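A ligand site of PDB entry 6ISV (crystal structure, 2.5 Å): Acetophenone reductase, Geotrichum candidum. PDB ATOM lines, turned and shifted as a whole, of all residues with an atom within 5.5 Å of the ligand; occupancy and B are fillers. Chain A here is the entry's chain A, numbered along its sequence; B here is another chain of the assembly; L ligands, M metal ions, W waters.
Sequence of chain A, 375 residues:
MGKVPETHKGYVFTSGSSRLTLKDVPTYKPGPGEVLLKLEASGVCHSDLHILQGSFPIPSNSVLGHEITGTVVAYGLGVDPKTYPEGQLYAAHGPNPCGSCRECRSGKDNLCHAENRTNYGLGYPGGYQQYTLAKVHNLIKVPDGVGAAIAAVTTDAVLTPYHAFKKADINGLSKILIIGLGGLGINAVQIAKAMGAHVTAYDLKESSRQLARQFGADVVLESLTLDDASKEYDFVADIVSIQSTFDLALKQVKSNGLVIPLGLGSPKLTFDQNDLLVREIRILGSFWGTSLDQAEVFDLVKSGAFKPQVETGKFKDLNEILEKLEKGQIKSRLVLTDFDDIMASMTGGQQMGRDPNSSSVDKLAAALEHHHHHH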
ATOM      1  N   VAL A  44      15.044   0.108   9.893  1.00  0.00           N
ATOM      2  CA  VAL A  44      14.921   1.552   9.986  1.00  0.00           C
ATOM      3  C   VAL A  44      15.977   2.058  10.954  1.00  0.00           C
ATOM      4  O   VAL A  44      15.942   1.737  12.151  1.00  0.00           O
ATOM      5  CB  VAL A  44      13.505   1.955  10.443  1.00  0.00           C
ATOM      6  CG1 VAL A  44      13.374   3.437  10.472  1.00  0.00           C
ATOM      7  CG2 VAL A  44      12.463   1.354   9.516  1.00  0.00           C
ATOM      8  N   CYS A  45      16.906   2.862  10.450  1.00  0.00           N
ATOM      9  CA  CYS A  45      18.073   3.345  11.178  1.00  0.00           C
ATOM     10  C   CYS A  45      17.974   4.844  11.457  1.00  0.00           C
ATOM     11  O   CYS A  45      17.533   5.613  10.596  1.00  0.00           O
ATOM     12  CB  CYS A  45      19.360   3.074  10.397  1.00  0.00           C
ATOM     13  SG  CYS A  45      20.857   3.500  11.269  1.00  0.00           S
ATOM     14  N   HIS A  46      18.411   5.257  12.655  1.00  0.00           N
ATOM     15  CA  HIS A  46      18.310   6.662  13.084  1.00  0.00           C
ATOM     16  C   HIS A  46      19.116   7.566  12.174  1.00  0.00           C
ATOM     17  O   HIS A  46      18.755   8.737  11.970  1.00  0.00           O
ATOM     18  CB  HIS A  46      18.764   6.806  14.548  1.00  0.00           C
ATOM     19  CG  HIS A  46      18.302   8.071  15.218  1.00  0.00           C
ATOM     20  ND1 HIS A  46      17.704   8.087  16.466  1.00  0.00           N
ATOM     21  CD2 HIS A  46      18.396   9.370  14.837  1.00  0.00           C
ATOM     22  CE1 HIS A  46      17.429   9.332  16.799  1.00  0.00           C
ATOM     23  NE2 HIS A  46      17.837  10.130  15.835  1.00  0.00           N
ATOM     24  N   SER A  47      20.214   7.045  11.610  1.00  0.00           N
ATOM     25  CA  SER A  47      20.929   7.797  10.575  1.00  0.00           C
ATOM     26  C   SER A  47      19.998   8.346   9.512  1.00  0.00           C
ATOM     27  O   SER A  47      20.300   9.366   8.890  1.00  0.00           O
ATOM     28  CB  SER A  47      21.983   6.913   9.912  1.00  0.00           C
ATOM     29  OG  SER A  47      22.647   6.116  10.860  1.00  0.00           O
ATOM     30  N   HIS A  50      18.823  11.490  10.638  1.00  0.00           N
ATOM     31  CA  HIS A  50      19.866  12.497  10.414  1.00  0.00           C
ATOM     32  C   HIS A  50      19.933  12.920   8.946  1.00  0.00           C
ATOM     33  O   HIS A  50      20.236  14.084   8.649  1.00  0.00           O
ATOM     34  CB  HIS A  50      21.229  11.983  10.886  1.00  0.00           C
ATOM     35  CG  HIS A  50      21.274  11.655  12.347  1.00  0.00           C
ATOM     36  ND1 HIS A  50      20.347  12.129  13.245  1.00  0.00           N
ATOM     37  CD2 HIS A  50      22.126  10.863  13.051  1.00  0.00           C
ATOM     38  CE1 HIS A  50      20.632  11.668  14.449  1.00  0.00           C
ATOM     39  NE2 HIS A  50      21.696  10.889  14.366  1.00  0.00           N
ATOM     40  N   HIS A  66      18.977   1.074   4.395  1.00  0.00           N
ATOM     41  CA  HIS A  66      20.275   0.427   4.260  1.00  0.00           C
ATOM     42  C   HIS A  66      20.425  -0.790   5.151  1.00  0.00           C
ATOM     43  O   HIS A  66      21.551  -1.293   5.292  1.00  0.00           O
ATOM     44  CB  HIS A  66      21.423   1.412   4.539  1.00  0.00           C
ATOM     45  CG  HIS A  66      21.380   2.045   5.903  1.00  0.00           C
ATOM     46  ND1 HIS A  66      20.626   3.167   6.168  1.00  0.00           N
ATOM     47  CD2 HIS A  66      22.006   1.725   7.049  1.00  0.00           C
ATOM     48  CE1 HIS A  66      20.795   3.505   7.433  1.00  0.00           C
ATOM     49  NE2 HIS A  66      21.629   2.644   7.994  1.00  0.00           N
ATOM     50  N   ASP A 156      23.509  -3.819  10.357  1.00  0.00           N
ATOM     51  CA  ASP A 156      23.890  -2.478  10.791  1.00  0.00           C
ATOM     52  C   ASP A 156      23.816  -2.376  12.312  1.00  0.00           C
ATOM     53  O   ASP A 156      24.859  -2.318  12.983  1.00  0.00           O
ATOM     54  CB  ASP A 156      22.983  -1.448  10.091  1.00  0.00           C
ATOM     55  CG  ASP A 156      23.240   0.001  10.528  1.00  0.00           C
ATOM     56  OD1 ASP A 156      24.334   0.298  11.077  1.00  0.00           O
ATOM     57  OD2 ASP A 156      22.317   0.839  10.323  1.00  0.00           O
ATOM     58  N   THR A 160      27.541  -2.688  13.222  1.00  0.00           N
ATOM     59  CA  THR A 160      28.302  -1.488  13.546  1.00  0.00           C
ATOM     60  C   THR A 160      28.868  -1.524  14.965  1.00  0.00           C
ATOM     61  O   THR A 160      30.090  -1.308  15.125  1.00  0.00           O
ATOM     62  CB  THR A 160      27.432  -0.238  13.325  1.00  0.00           C
ATOM     63  OG1 THR A 160      27.024  -0.139  11.943  1.00  0.00           O
ATOM     64  CG2 THR A 160      28.197   1.015  13.738  1.00  0.00           C
ATOM     65  N   ILE A 179      26.724   4.499  26.247  1.00  0.00           N
ATOM     66  CA  ILE A 179      25.707   5.545  26.314  1.00  0.00           C
ATOM     67  C   ILE A 179      24.830   5.425  25.080  1.00  0.00           C
ATOM     68  O   ILE A 179      25.320   5.500  23.944  1.00  0.00           O
ATOM     69  CB  ILE A 179      26.314   6.945  26.428  1.00  0.00           C
ATOM     70  CG1 ILE A 179      27.371   6.977  27.528  1.00  0.00           C
ATOM     71  CG2 ILE A 179      25.220   7.956  26.722  1.00  0.00           C
ATOM     72  CD1 ILE A 179      27.856   8.350  27.845  1.00  0.00           C
ATOM     73  N   GLY A 180      23.534   5.234  25.301  1.00  0.00           N
ATOM     74  CA  GLY A 180      22.615   5.030  24.210  1.00  0.00           C
ATOM     75  C   GLY A 180      22.255   3.572  24.045  1.00  0.00           C
ATOM     76  O   GLY A 180      23.109   2.728  23.703  1.00  0.00           O
ATOM     77  N   LEU A 181      20.975   3.256  24.300  1.00  0.00           N
ATOM     78  CA  LEU A 181      20.438   1.898  24.329  1.00  0.00           C
ATOM     79  C   LEU A 181      19.213   1.779  23.438  1.00  0.00           C
ATOM     80  O   LEU A 181      18.167   1.268  23.822  1.00  0.00           O
ATOM     81  CB  LEU A 181      20.070   1.519  25.757  1.00  0.00           C
ATOM     82  CG  LEU A 181      21.212   1.650  26.741  1.00  0.00           C
ATOM     83  CD1 LEU A 181      20.691   1.375  28.133  1.00  0.00           C
ATOM     84  CD2 LEU A 181      22.311   0.652  26.370  1.00  0.00           C
ATOM     85  N   GLY A 182      19.316   2.261  22.211  1.00  0.00           N
ATOM     86  CA  GLY A 182      18.309   1.969  21.218  1.00  0.00           C
ATOM     87  C   GLY A 182      18.682   0.751  20.408  1.00  0.00           C
ATOM     88  O   GLY A 182      19.185  -0.249  20.931  1.00  0.00           O
ATOM     89  N   GLY A 183      18.471   0.851  19.098  1.00  0.00           N
ATOM     90  CA  GLY A 183      18.678  -0.297  18.225  1.00  0.00           C
ATOM     91  C   GLY A 183      20.121  -0.768  18.212  1.00  0.00           C
ATOM     92  O   GLY A 183      20.404  -1.964  18.395  1.00  0.00           O
ATOM     93  N   LEU A 184      21.058   0.153  17.980  1.00  0.00           N
ATOM     94  CA  LEU A 184      22.467  -0.186  18.146  1.00  0.00           C
ATOM     95  C   LEU A 184      22.772  -0.574  19.583  1.00  0.00           C
ATOM     96  O   LEU A 184      23.409  -1.607  19.830  1.00  0.00           O
ATOM     97  CB  LEU A 184      23.360   0.981  17.698  1.00  0.00           C
ATOM     98  CG  LEU A 184      23.770   0.977  16.227  1.00  0.00           C
ATOM     99  CD1 LEU A 184      22.541   1.159  15.349  1.00  0.00           C
ATOM    100  CD2 LEU A 184      24.790   2.065  15.923  1.00  0.00           C
ATOM    101  N   GLY A 185      22.298   0.221  20.548  1.00  0.00           N
ATOM    102  CA  GLY A 185      22.781   0.113  21.926  1.00  0.00           C
ATOM    103  C   GLY A 185      22.519  -1.231  22.582  1.00  0.00           C
ATOM    104  O   GLY A 185      23.391  -1.770  23.288  1.00  0.00           O
ATOM    105  N   TYR A 202      23.737   3.413  30.110  1.00  0.00           N
ATOM    106  CA  TYR A 202      22.873   4.542  30.391  1.00  0.00           C
ATOM    107  C   TYR A 202      22.068   4.899  29.155  1.00  0.00           C
ATOM    108  O   TYR A 202      22.634   4.971  28.044  1.00  0.00           O
ATOM    109  CB  TYR A 202      23.663   5.759  30.850  1.00  0.00           C
ATOM    110  CG  TYR A 202      22.780   6.975  31.044  1.00  0.00           C
ATOM    111  CD1 TYR A 202      21.848   7.017  32.062  1.00  0.00           C
ATOM    112  CD2 TYR A 202      22.866   8.067  30.190  1.00  0.00           C
ATOM    113  CE1 TYR A 202      21.039   8.114  32.239  1.00  0.00           C
ATOM    114  CE2 TYR A 202      22.051   9.169  30.356  1.00  0.00           C
ATOM    115  CZ  TYR A 202      21.138   9.188  31.378  1.00  0.00           C
ATOM    116  OH  TYR A 202      20.325  10.288  31.568  1.00  0.00           O
ATOM    117  N   ASP A 203      20.766   5.130  29.346  1.00  0.00           N
ATOM    118  CA  ASP A 203      19.854   5.684  28.357  1.00  0.00           C
ATOM    119  C   ASP A 203      18.838   6.525  29.119  1.00  0.00           C
ATOM    120  O   ASP A 203      18.677   6.373  30.334  1.00  0.00           O
ATOM    121  CB  ASP A 203      19.173   4.570  27.552  1.00  0.00           C
ATOM    122  CG  ASP A 203      18.433   5.074  26.326  1.00  0.00           C
ATOM    123  OD1 ASP A 203      17.462   5.827  26.475  1.00  0.00           O
ATOM    124  OD2 ASP A 203      18.826   4.706  25.207  1.00  0.00           O
ATOM    125  N   LEU A 204      18.161   7.421  28.410  1.00  0.00           N
ATOM    126  CA  LEU A 204      17.084   8.183  29.033  1.00  0.00           C
ATOM    127  C   LEU A 204      15.823   7.349  29.169  1.00  0.00           C
ATOM    128  O   LEU A 204      15.123   7.448  30.197  1.00  0.00           O
ATOM    129  CB  LEU A 204      16.790   9.440  28.230  1.00  0.00           C
ATOM    130  CG  LEU A 204      17.984  10.293  27.854  1.00  0.00           C
ATOM    131  CD1 LEU A 204      17.655  11.228  26.679  1.00  0.00           C
ATOM    132  CD2 LEU A 204      18.436  11.071  29.080  1.00  0.00           C
ATOM    133  N   LYS A 205      15.500   6.555  28.156  1.00  0.00           N
ATOM    134  CA  LYS A 205      14.279   5.752  28.177  1.00  0.00           C
ATOM    135  C   LYS A 205      14.384   4.676  29.250  1.00  0.00           C
ATOM    136  O   LYS A 205      15.395   3.964  29.333  1.00  0.00           O
ATOM    137  CB  LYS A 205      14.026   5.093  26.814  1.00  0.00           C
ATOM    138  CG  LYS A 205      13.719   6.060  25.669  1.00  0.00           C
ATOM    139  CD  LYS A 205      13.480   5.328  24.350  1.00  0.00           C
ATOM    140  CE  LYS A 205      12.408   4.259  24.496  1.00  0.00           C
ATOM    141  NZ  LYS A 205      11.981   3.731  23.160  1.00  0.00           N
ATOM    142  N   SER A 208      14.324   1.257  27.653  1.00  0.00           N
ATOM    143  CA  SER A 208      15.662   0.978  27.127  1.00  0.00           C
ATOM    144  C   SER A 208      16.601   0.532  28.237  1.00  0.00           C
ATOM    145  O   SER A 208      17.375  -0.424  28.054  1.00  0.00           O
ATOM    146  CB  SER A 208      16.218   2.219  26.431  1.00  0.00           C
ATOM    147  OG  SER A 208      15.654   2.396  25.147  1.00  0.00           O
ATOM    148  N   ILE A 239      27.078   6.061  21.855  1.00  0.00           N
ATOM    149  CA  ILE A 239      26.245   5.775  20.689  1.00  0.00           C
ATOM    150  C   ILE A 239      25.131   6.810  20.574  1.00  0.00           C
ATOM    151  O   ILE A 239      24.147   6.625  19.838  1.00  0.00           O
ATOM    152  CB  ILE A 239      25.680   4.349  20.762  1.00  0.00           C
ATOM    153  CG1 ILE A 239      26.681   3.421  21.477  1.00  0.00           C
ATOM    154  CG2 ILE A 239      25.388   3.827  19.339  1.00  0.00           C
ATOM    155  CD1 ILE A 239      26.282   1.936  21.520  1.00  0.00           C
ATOM    156  N   VAL A 240      25.264   7.910  21.310  1.00  0.00           N
ATOM    157  CA  VAL A 240      24.469   9.107  21.080  1.00  0.00           C
ATOM    158  C   VAL A 240      25.272  10.157  20.319  1.00  0.00           C
ATOM    159  O   VAL A 240      24.844  10.633  19.262  1.00  0.00           O
ATOM    160  CB  VAL A 240      23.950   9.681  22.408  1.00  0.00           C
ATOM    161  CG1 VAL A 240      22.991  10.856  22.130  1.00  0.00           C
ATOM    162  CG2 VAL A 240      23.291   8.579  23.237  1.00  0.00           C
ATOM    163  N   ILE A 242      26.053  13.323  20.968  1.00  0.00           N
ATOM    164  CA  ILE A 242      25.881  14.777  21.051  1.00  0.00           C
ATOM    165  C   ILE A 242      26.911  15.303  22.036  1.00  0.00           C
ATOM    166  O   ILE A 242      27.711  14.530  22.582  1.00  0.00           O
ATOM    167  CB  ILE A 242      24.453  15.177  21.451  1.00  0.00           C
ATOM    168  CG1 ILE A 242      24.068  14.577  22.810  1.00  0.00           C
ATOM    169  CG2 ILE A 242      23.469  14.834  20.317  1.00  0.00           C
ATOM    170  CD1 ILE A 242      22.680  14.971  23.309  1.00  0.00           C
ATOM    171  N   SER A 244      26.535  16.790  25.113  1.00  0.00           N
ATOM    172  CA  SER A 244      26.213  16.245  26.419  1.00  0.00           C
ATOM    173  C   SER A 244      26.883  14.881  26.654  1.00  0.00           C
ATOM    174  O   SER A 244      27.664  14.696  27.607  1.00  0.00           O
ATOM    175  CB  SER A 244      24.684  16.143  26.529  1.00  0.00           C
ATOM    176  OG  SER A 244      24.284  15.176  27.480  1.00  0.00           O
ATOM    177  N   THR A 245      26.597  13.934  25.765  1.00  0.00           N
ATOM    178  CA  THR A 245      27.094  12.571  25.950  1.00  0.00           C
ATOM    179  C   THR A 245      28.593  12.493  25.720  1.00  0.00           C
ATOM    180  O   THR A 245      29.275  11.750  26.433  1.00  0.00           O
ATOM    181  CB  THR A 245      26.356  11.620  25.021  1.00  0.00           C
ATOM    182  OG1 THR A 245      26.598  12.009  23.655  1.00  0.00           O
ATOM    183  CG2 THR A 245      24.865  11.703  25.321  1.00  0.00           C
ATOM    184  N   LEU A 262      30.289   6.596  18.520  1.00  0.00           N
ATOM    185  CA  LEU A 262      29.657   5.801  17.482  1.00  0.00           C
ATOM    186  C   LEU A 262      28.447   6.493  16.859  1.00  0.00           C
ATOM    187  O   LEU A 262      28.116   6.202  15.706  1.00  0.00           O
ATOM    188  CB  LEU A 262      29.241   4.443  18.061  1.00  0.00           C
ATOM    189  CG  LEU A 262      29.110   3.198  17.176  1.00  0.00           C
ATOM    190  CD1 LEU A 262      30.296   2.955  16.227  1.00  0.00           C
ATOM    191  CD2 LEU A 262      28.909   1.998  18.078  1.00  0.00           C
ATOM    192  N   GLY A 263      27.789   7.425  17.572  1.00  0.00           N
ATOM    193  CA  GLY A 263      26.577   8.041  17.073  1.00  0.00           C
ATOM    194  C   GLY A 263      26.832   9.164  16.099  1.00  0.00           C
ATOM    195  O   GLY A 263      27.969   9.567  15.839  1.00  0.00           O
ATOM    196  N   LEU A 264      25.737   9.672  15.518  1.00  0.00           N
ATOM    197  CA  LEU A 264      25.756  10.878  14.692  1.00  0.00           C
ATOM    198  C   LEU A 264      24.822  11.942  15.269  1.00  0.00           C
ATOM    199  O   LEU A 264      24.237  12.734  14.524  1.00  0.00           O
ATOM    200  CB  LEU A 264      25.375  10.570  13.245  1.00  0.00           C
ATOM    201  CG  LEU A 264      26.385   9.773  12.410  1.00  0.00           C
ATOM    202  CD1 LEU A 264      25.784   9.275  11.094  1.00  0.00           C
ATOM    203  CD2 LEU A 264      27.616  10.613  12.141  1.00  0.00           C
ATOM    204  N   GLY A 265      24.689  11.978  16.611  1.00  0.00           N
ATOM    205  CA  GLY A 265      23.724  12.881  17.231  1.00  0.00           C
ATOM    206  C   GLY A 265      23.946  14.341  16.893  1.00  0.00           C
ATOM    207  O   GLY A 265      23.000  15.140  16.880  1.00  0.00           O
ATOM    208  N   SER A 286      34.565   4.899  13.957  1.00  0.00           N
ATOM    209  CA  SER A 286      34.276   3.526  13.560  1.00  0.00           C
ATOM    210  C   SER A 286      32.966   3.517  12.776  1.00  0.00           C
ATOM    211  O   SER A 286      31.944   4.002  13.267  1.00  0.00           O
ATOM    212  CB  SER A 286      34.186   2.617  14.790  1.00  0.00           C
ATOM    213  OG  SER A 286      33.623   1.353  14.469  1.00  0.00           O
ATOM    214  N   PHE A 287      32.986   2.959  11.555  1.00  0.00           N
ATOM    215  CA  PHE A 287      31.925   3.149  10.555  1.00  0.00           C
ATOM    216  C   PHE A 287      31.451   1.814   9.990  1.00  0.00           C
ATOM    217  O   PHE A 287      32.247   1.085   9.390  1.00  0.00           O
ATOM    218  CB  PHE A 287      32.452   4.042   9.434  1.00  0.00           C
ATOM    219  CG  PHE A 287      31.486   4.236   8.281  1.00  0.00           C
ATOM    220  CD1 PHE A 287      30.258   4.847   8.455  1.00  0.00           C
ATOM    221  CD2 PHE A 287      31.848   3.833   7.000  1.00  0.00           C
ATOM    222  CE1 PHE A 287      29.390   5.033   7.383  1.00  0.00           C
ATOM    223  CE2 PHE A 287      31.001   4.031   5.931  1.00  0.00           C
ATOM    224  CZ  PHE A 287      29.769   4.623   6.116  1.00  0.00           C
ATOM    225  N   TRP A 288      30.143   1.517  10.110  1.00  0.00           N
ATOM    226  CA  TRP A 288      29.508   0.297   9.565  1.00  0.00           C
ATOM    227  C   TRP A 288      30.281  -0.937  10.077  1.00  0.00           C
ATOM    228  O   TRP A 288      30.705  -0.973  11.230  1.00  0.00           O
ATOM    229  CB  TRP A 288      29.496   0.296   8.031  1.00  0.00           C
ATOM    230  CG  TRP A 288      28.254   0.725   7.191  1.00  0.00           C
ATOM    231  CD1 TRP A 288      28.199   1.764   6.249  1.00  0.00           C
ATOM    232  CD2 TRP A 288      26.969   0.082   7.108  1.00  0.00           C
ATOM    233  NE1 TRP A 288      26.964   1.822   5.626  1.00  0.00           N
ATOM    234  CE2 TRP A 288      26.185   0.806   6.130  1.00  0.00           C
ATOM    235  CE3 TRP A 288      26.390  -1.004   7.761  1.00  0.00           C
ATOM    236  CZ2 TRP A 288      24.872   0.477   5.821  1.00  0.00           C
ATOM    237  CZ3 TRP A 288      25.086  -1.339   7.426  1.00  0.00           C
ATOM    238  CH2 TRP A 288      24.344  -0.606   6.483  1.00  0.00           C
ATOM    239  N   LEU A 325      10.282   7.291  15.811  1.00  0.00           N
ATOM    240  CA  LEU A 325      11.665   7.085  16.196  1.00  0.00           C
ATOM    241  C   LEU A 325      12.329   8.390  16.632  1.00  0.00           C
ATOM    242  O   LEU A 325      13.077   8.408  17.611  1.00  0.00           O
ATOM    243  CB  LEU A 325      12.442   6.451  15.035  1.00  0.00           C
ATOM    244  CG  LEU A 325      13.817   5.881  15.371  1.00  0.00           C
ATOM    245  CD1 LEU A 325      13.673   4.628  16.221  1.00  0.00           C
ATOM    246  CD2 LEU A 325      14.588   5.584  14.108  1.00  0.00           C
ATOM    247  N   SER A 332      13.098  -0.720  20.425  1.00  0.00           N
ATOM    248  CA  SER A 332      14.490  -0.831  20.008  1.00  0.00           C
ATOM    249  C   SER A 332      14.591  -0.486  18.523  1.00  0.00           C
ATOM    250  O   SER A 332      14.624   0.690  18.150  1.00  0.00           O
ATOM    251  CB  SER A 332      15.034  -2.228  20.300  1.00  0.00           C
ATOM    252  OG  SER A 332      16.423  -2.169  20.604  1.00  0.00           O
ATOM    253  N   ARG A 333      14.635  -1.511  17.676  1.00  0.00           N
ATOM    254  CA  ARG A 333      14.670  -1.285  16.249  1.00  0.00           C
ATOM    255  C   ARG A 333      13.386  -1.797  15.612  1.00  0.00           C
ATOM    256  O   ARG A 333      12.842  -2.828  16.012  1.00  0.00           O
ATOM    257  CB  ARG A 333      15.889  -1.954  15.591  1.00  0.00           C
ATOM    258  CG  ARG A 333      16.239  -1.238  14.285  1.00  0.00           C
ATOM    259  CD  ARG A 333      17.578  -1.563  13.815  1.00  0.00           C
ATOM    260  NE  ARG A 333      18.265  -0.475  13.151  1.00  0.00           N
ATOM    261  CZ  ARG A 333      18.915   0.476  13.809  1.00  0.00           C
ATOM    262  NH1 ARG A 333      18.923   0.451  15.134  1.00  0.00           N
ATOM    263  NH2 ARG A 333      19.550   1.427  13.159  1.00  0.00           N
ATOM    264  N   LEU B 277      33.878   9.896  11.773  1.00  0.00           N
ATOM    265  CA  LEU B 277      33.218   8.593  11.794  1.00  0.00           C
ATOM    266  C   LEU B 277      33.375   7.868  10.459  1.00  0.00           C
ATOM    267  O   LEU B 277      33.841   6.724  10.416  1.00  0.00           O
ATOM    268  CB  LEU B 277      31.752   8.796  12.159  1.00  0.00           C
ATOM    269  CG  LEU B 277      30.844   7.570  12.333  1.00  0.00           C
ATOM    270  CD1 LEU B 277      29.874   7.772  13.484  1.00  0.00           C
ATOM    271  CD2 LEU B 277      30.097   7.308  11.037  1.00  0.00           C
HETATM  272  P1  LIG L   1      17.516   4.555  18.158  1.00  0.00           P
HETATM  273  O1  LIG L   1      16.488   5.552  17.783  1.00  0.00           O
HETATM  274  O2  LIG L   1      17.239   3.121  17.938  1.00  0.00           O
HETATM  275  O3  LIG L   1      17.843   4.746  19.721  1.00  0.00           O
HETATM  276  C1  LIG L   1      18.806   5.703  20.167  1.00  0.00           C
HETATM  277  C2  LIG L   1      18.808   5.757  21.708  1.00  0.00           C
HETATM  278  O4  LIG L   1      19.532   6.970  22.079  1.00  0.00           O
HETATM  279  C3  LIG L   1      17.394   5.916  22.290  1.00  0.00           C
HETATM  280  O5  LIG L   1      17.136   4.921  23.287  1.00  0.00           O
HETATM  281  C4  LIG L   1      17.545   7.257  22.969  1.00  0.00           C
HETATM  282  O6  LIG L   1      16.745   7.297  24.160  1.00  0.00           O
HETATM  283  C5  LIG L   1      18.993   7.250  23.338  1.00  0.00           C
HETATM  284  N1  LIG L   1      19.442   8.613  23.698  1.00  0.00           N
HETATM  285  C6  LIG L   1      19.252   9.703  22.945  1.00  0.00           C
HETATM  286  N2  LIG L   1      19.799  10.739  23.572  1.00  0.00           N
HETATM  287  C7  LIG L   1      20.323  10.301  24.727  1.00  0.00           C
HETATM  288  C8  LIG L   1      20.971  10.937  25.699  1.00  0.00           C
HETATM  289  N3  LIG L   1      21.144  12.245  25.555  1.00  0.00           N
HETATM  290  N4  LIG L   1      21.415  10.291  26.784  1.00  0.00           N
HETATM  291  C9  LIG L   1      21.209   8.915  26.895  1.00  0.00           C
HETATM  292  N5  LIG L   1      20.521   8.269  25.851  1.00  0.00           N
HETATM  293  C10 LIG L   1      20.101   8.983  24.796  1.00  0.00           C
HETATM  294  O7  LIG L   1      18.931   4.994  17.454  1.00  0.00           O
HETATM  295  P2  LIG L   1      19.949   3.956  16.723  1.00  0.00           P
HETATM  296  O8  LIG L   1      19.359   3.538  15.415  1.00  0.00           O
HETATM  297  O9  LIG L   1      20.394   2.949  17.701  1.00  0.00           O
HETATM  298  O10 LIG L   1      21.213   4.884  16.399  1.00  0.00           O
HETATM  299  C11 LIG L   1      21.850   5.684  17.391  1.00  0.00           C
HETATM  300  C12 LIG L   1      22.986   6.482  16.742  1.00  0.00           C
HETATM  301  O11 LIG L   1      23.824   5.532  15.993  1.00  0.00           O
HETATM  302  C13 LIG L   1      22.477   7.455  15.667  1.00  0.00           C
HETATM  303  O12 LIG L   1      23.255   8.660  15.722  1.00  0.00           O
HETATM  304  C14 LIG L   1      22.846   6.666  14.415  1.00  0.00           C
HETATM  305  O13 LIG L   1      22.885   7.517  13.266  1.00  0.00           O
HETATM  306  C15 LIG L   1      24.202   6.191  14.785  1.00  0.00           C
HETATM  307  N6  LIG L   1      24.782   5.175  13.822  1.00  0.00           N
HETATM  308  C16 LIG L   1      26.184   5.110  13.603  1.00  0.00           C
HETATM  309  C17 LIG L   1      26.745   4.173  12.737  1.00  0.00           C
HETATM  310  C18 LIG L   1      28.134   4.146  12.528  1.00  0.00           C
HETATM  311  O14 LIG L   1      28.921   4.502  13.397  1.00  0.00           O
HETATM  312  N7  LIG L   1      28.515   3.687  11.341  1.00  0.00           N
HETATM  313  C19 LIG L   1      25.907   3.284  12.080  1.00  0.00           C
HETATM  314  C20 LIG L   1      24.530   3.316  12.285  1.00  0.00           C
HETATM  315  C21 LIG L   1      23.957   4.248  13.155  1.00  0.00           C
HETATM  316 ZN    ZN M   1      22.649   2.894   9.824  1.00  0.00          ZN
HETATM  317  O   HOH W   1      22.043   9.444  18.725  1.00  0.00           O
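O of Leu 262 sits close to O14 of the ligand (3.0 Å).
O of Ser 286 lies close to O14 of the ligand (3.1 Å).
A nitrogen (N7) of the ligand lies close to the backbone NH (N) of Trp 288 (3.0 Å).
Merely in contact with the ligand: Cys 45 (3.7 Å), Asp 156 (3.3 Å), Thr 160 (3.4 Å), Leu 181 (3.8 Å), Gly 182 (3.2 Å), Tyr 202 (3.6 Å), Leu 204 (3.4 Å), Lys 205 (3.6 Å), Ile 239 (3.3 Å), Val 240 (3.5 Å), Ile 242 (3.9 Å), Thr 245 (3.8 Å), Gly 263 (3.6 Å), Gly 265 (3.7 Å), Phe 287 (3.5 Å), Leu 325 (3.3 Å), Ser 332 (3.6 Å) and Leu 277 of chain B (3.4 Å).
Water W1 bridges the backbone carbonyl oxygen of Val 240 (3.1 Å) and an oxygen (O12) of the ligand (3.3 Å).
OD2 of Asp 203 sits at hydrogen-bond distance from O5 of the ligand, at 2.6 Å.
O5 of the ligand lies within hydrogen-bond range of OG of Ser 208, 3.5 Å away.
An oxygen (O13) of the ligand sits at hydrogen-bond distance from the backbone NH of Ser 47 (3.2 Å).
The guanidinium group of Arg 333 lies within salt-bridge range of an oxygen (O8) of the ligand (3.1 Å).
N of Gly 183 is in hydrogen-bond range of O2 of the ligand, at 2.8 Å.
The backbone NH (N) of His 46 is in hydrogen-bond range of an oxygen (O8) of the ligand, at 3.4 Å.
An oxygen (O9) of the ligand is in hydrogen-bond range of the backbone NH (N) of Leu 184.
ND1 of His 46 is in hydrogen-bond range of O1 of the ligand.
A ring nitrogen (NE2) of His 50 lies within hydrogen-bond range of an oxygen (O12) of the ligand, at 3.0 Å.
The backbone NH (N) of Leu 264 lies within hydrogen-bond range of an oxygen (O12) of the ligand (2.7 Å).
O13 of the ligand lies within hydrogen-bond range of OG of Ser 47 (2.8 Å).
O of Tyr 202 lies within hydrogen-bond range of N of Gly 180.
NH2 of Arg 333 sits close to SG of Cys 45.
NE of Arg 333 sits at hydrogen-bond distance from O of Val 44, 3.4 Å away.
The backbone NH (N) of Gly 265 sits at hydrogen-bond distance from the backbone carbonyl oxygen (O) of Val 240 (3.0 Å).
The side-chain hydroxyl (OG) of Ser 47 sits close to the side-chain sulfur (SG) of Cys 45 (3.2 Å).
The side-chain hydroxyl (OG1) of Thr 245 sits at hydrogen-bond distance from the backbone carbonyl oxygen (O) of Ile 242.
The side-chain carboxylate of Asp 203 lies within hydrogen-bond range of the backbone NH of Lys 205 (2.7 Å).
The backbone NH (N) of Ile 239 sits at hydrogen-bond distance from the backbone carbonyl oxygen (O) of Ile 179.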
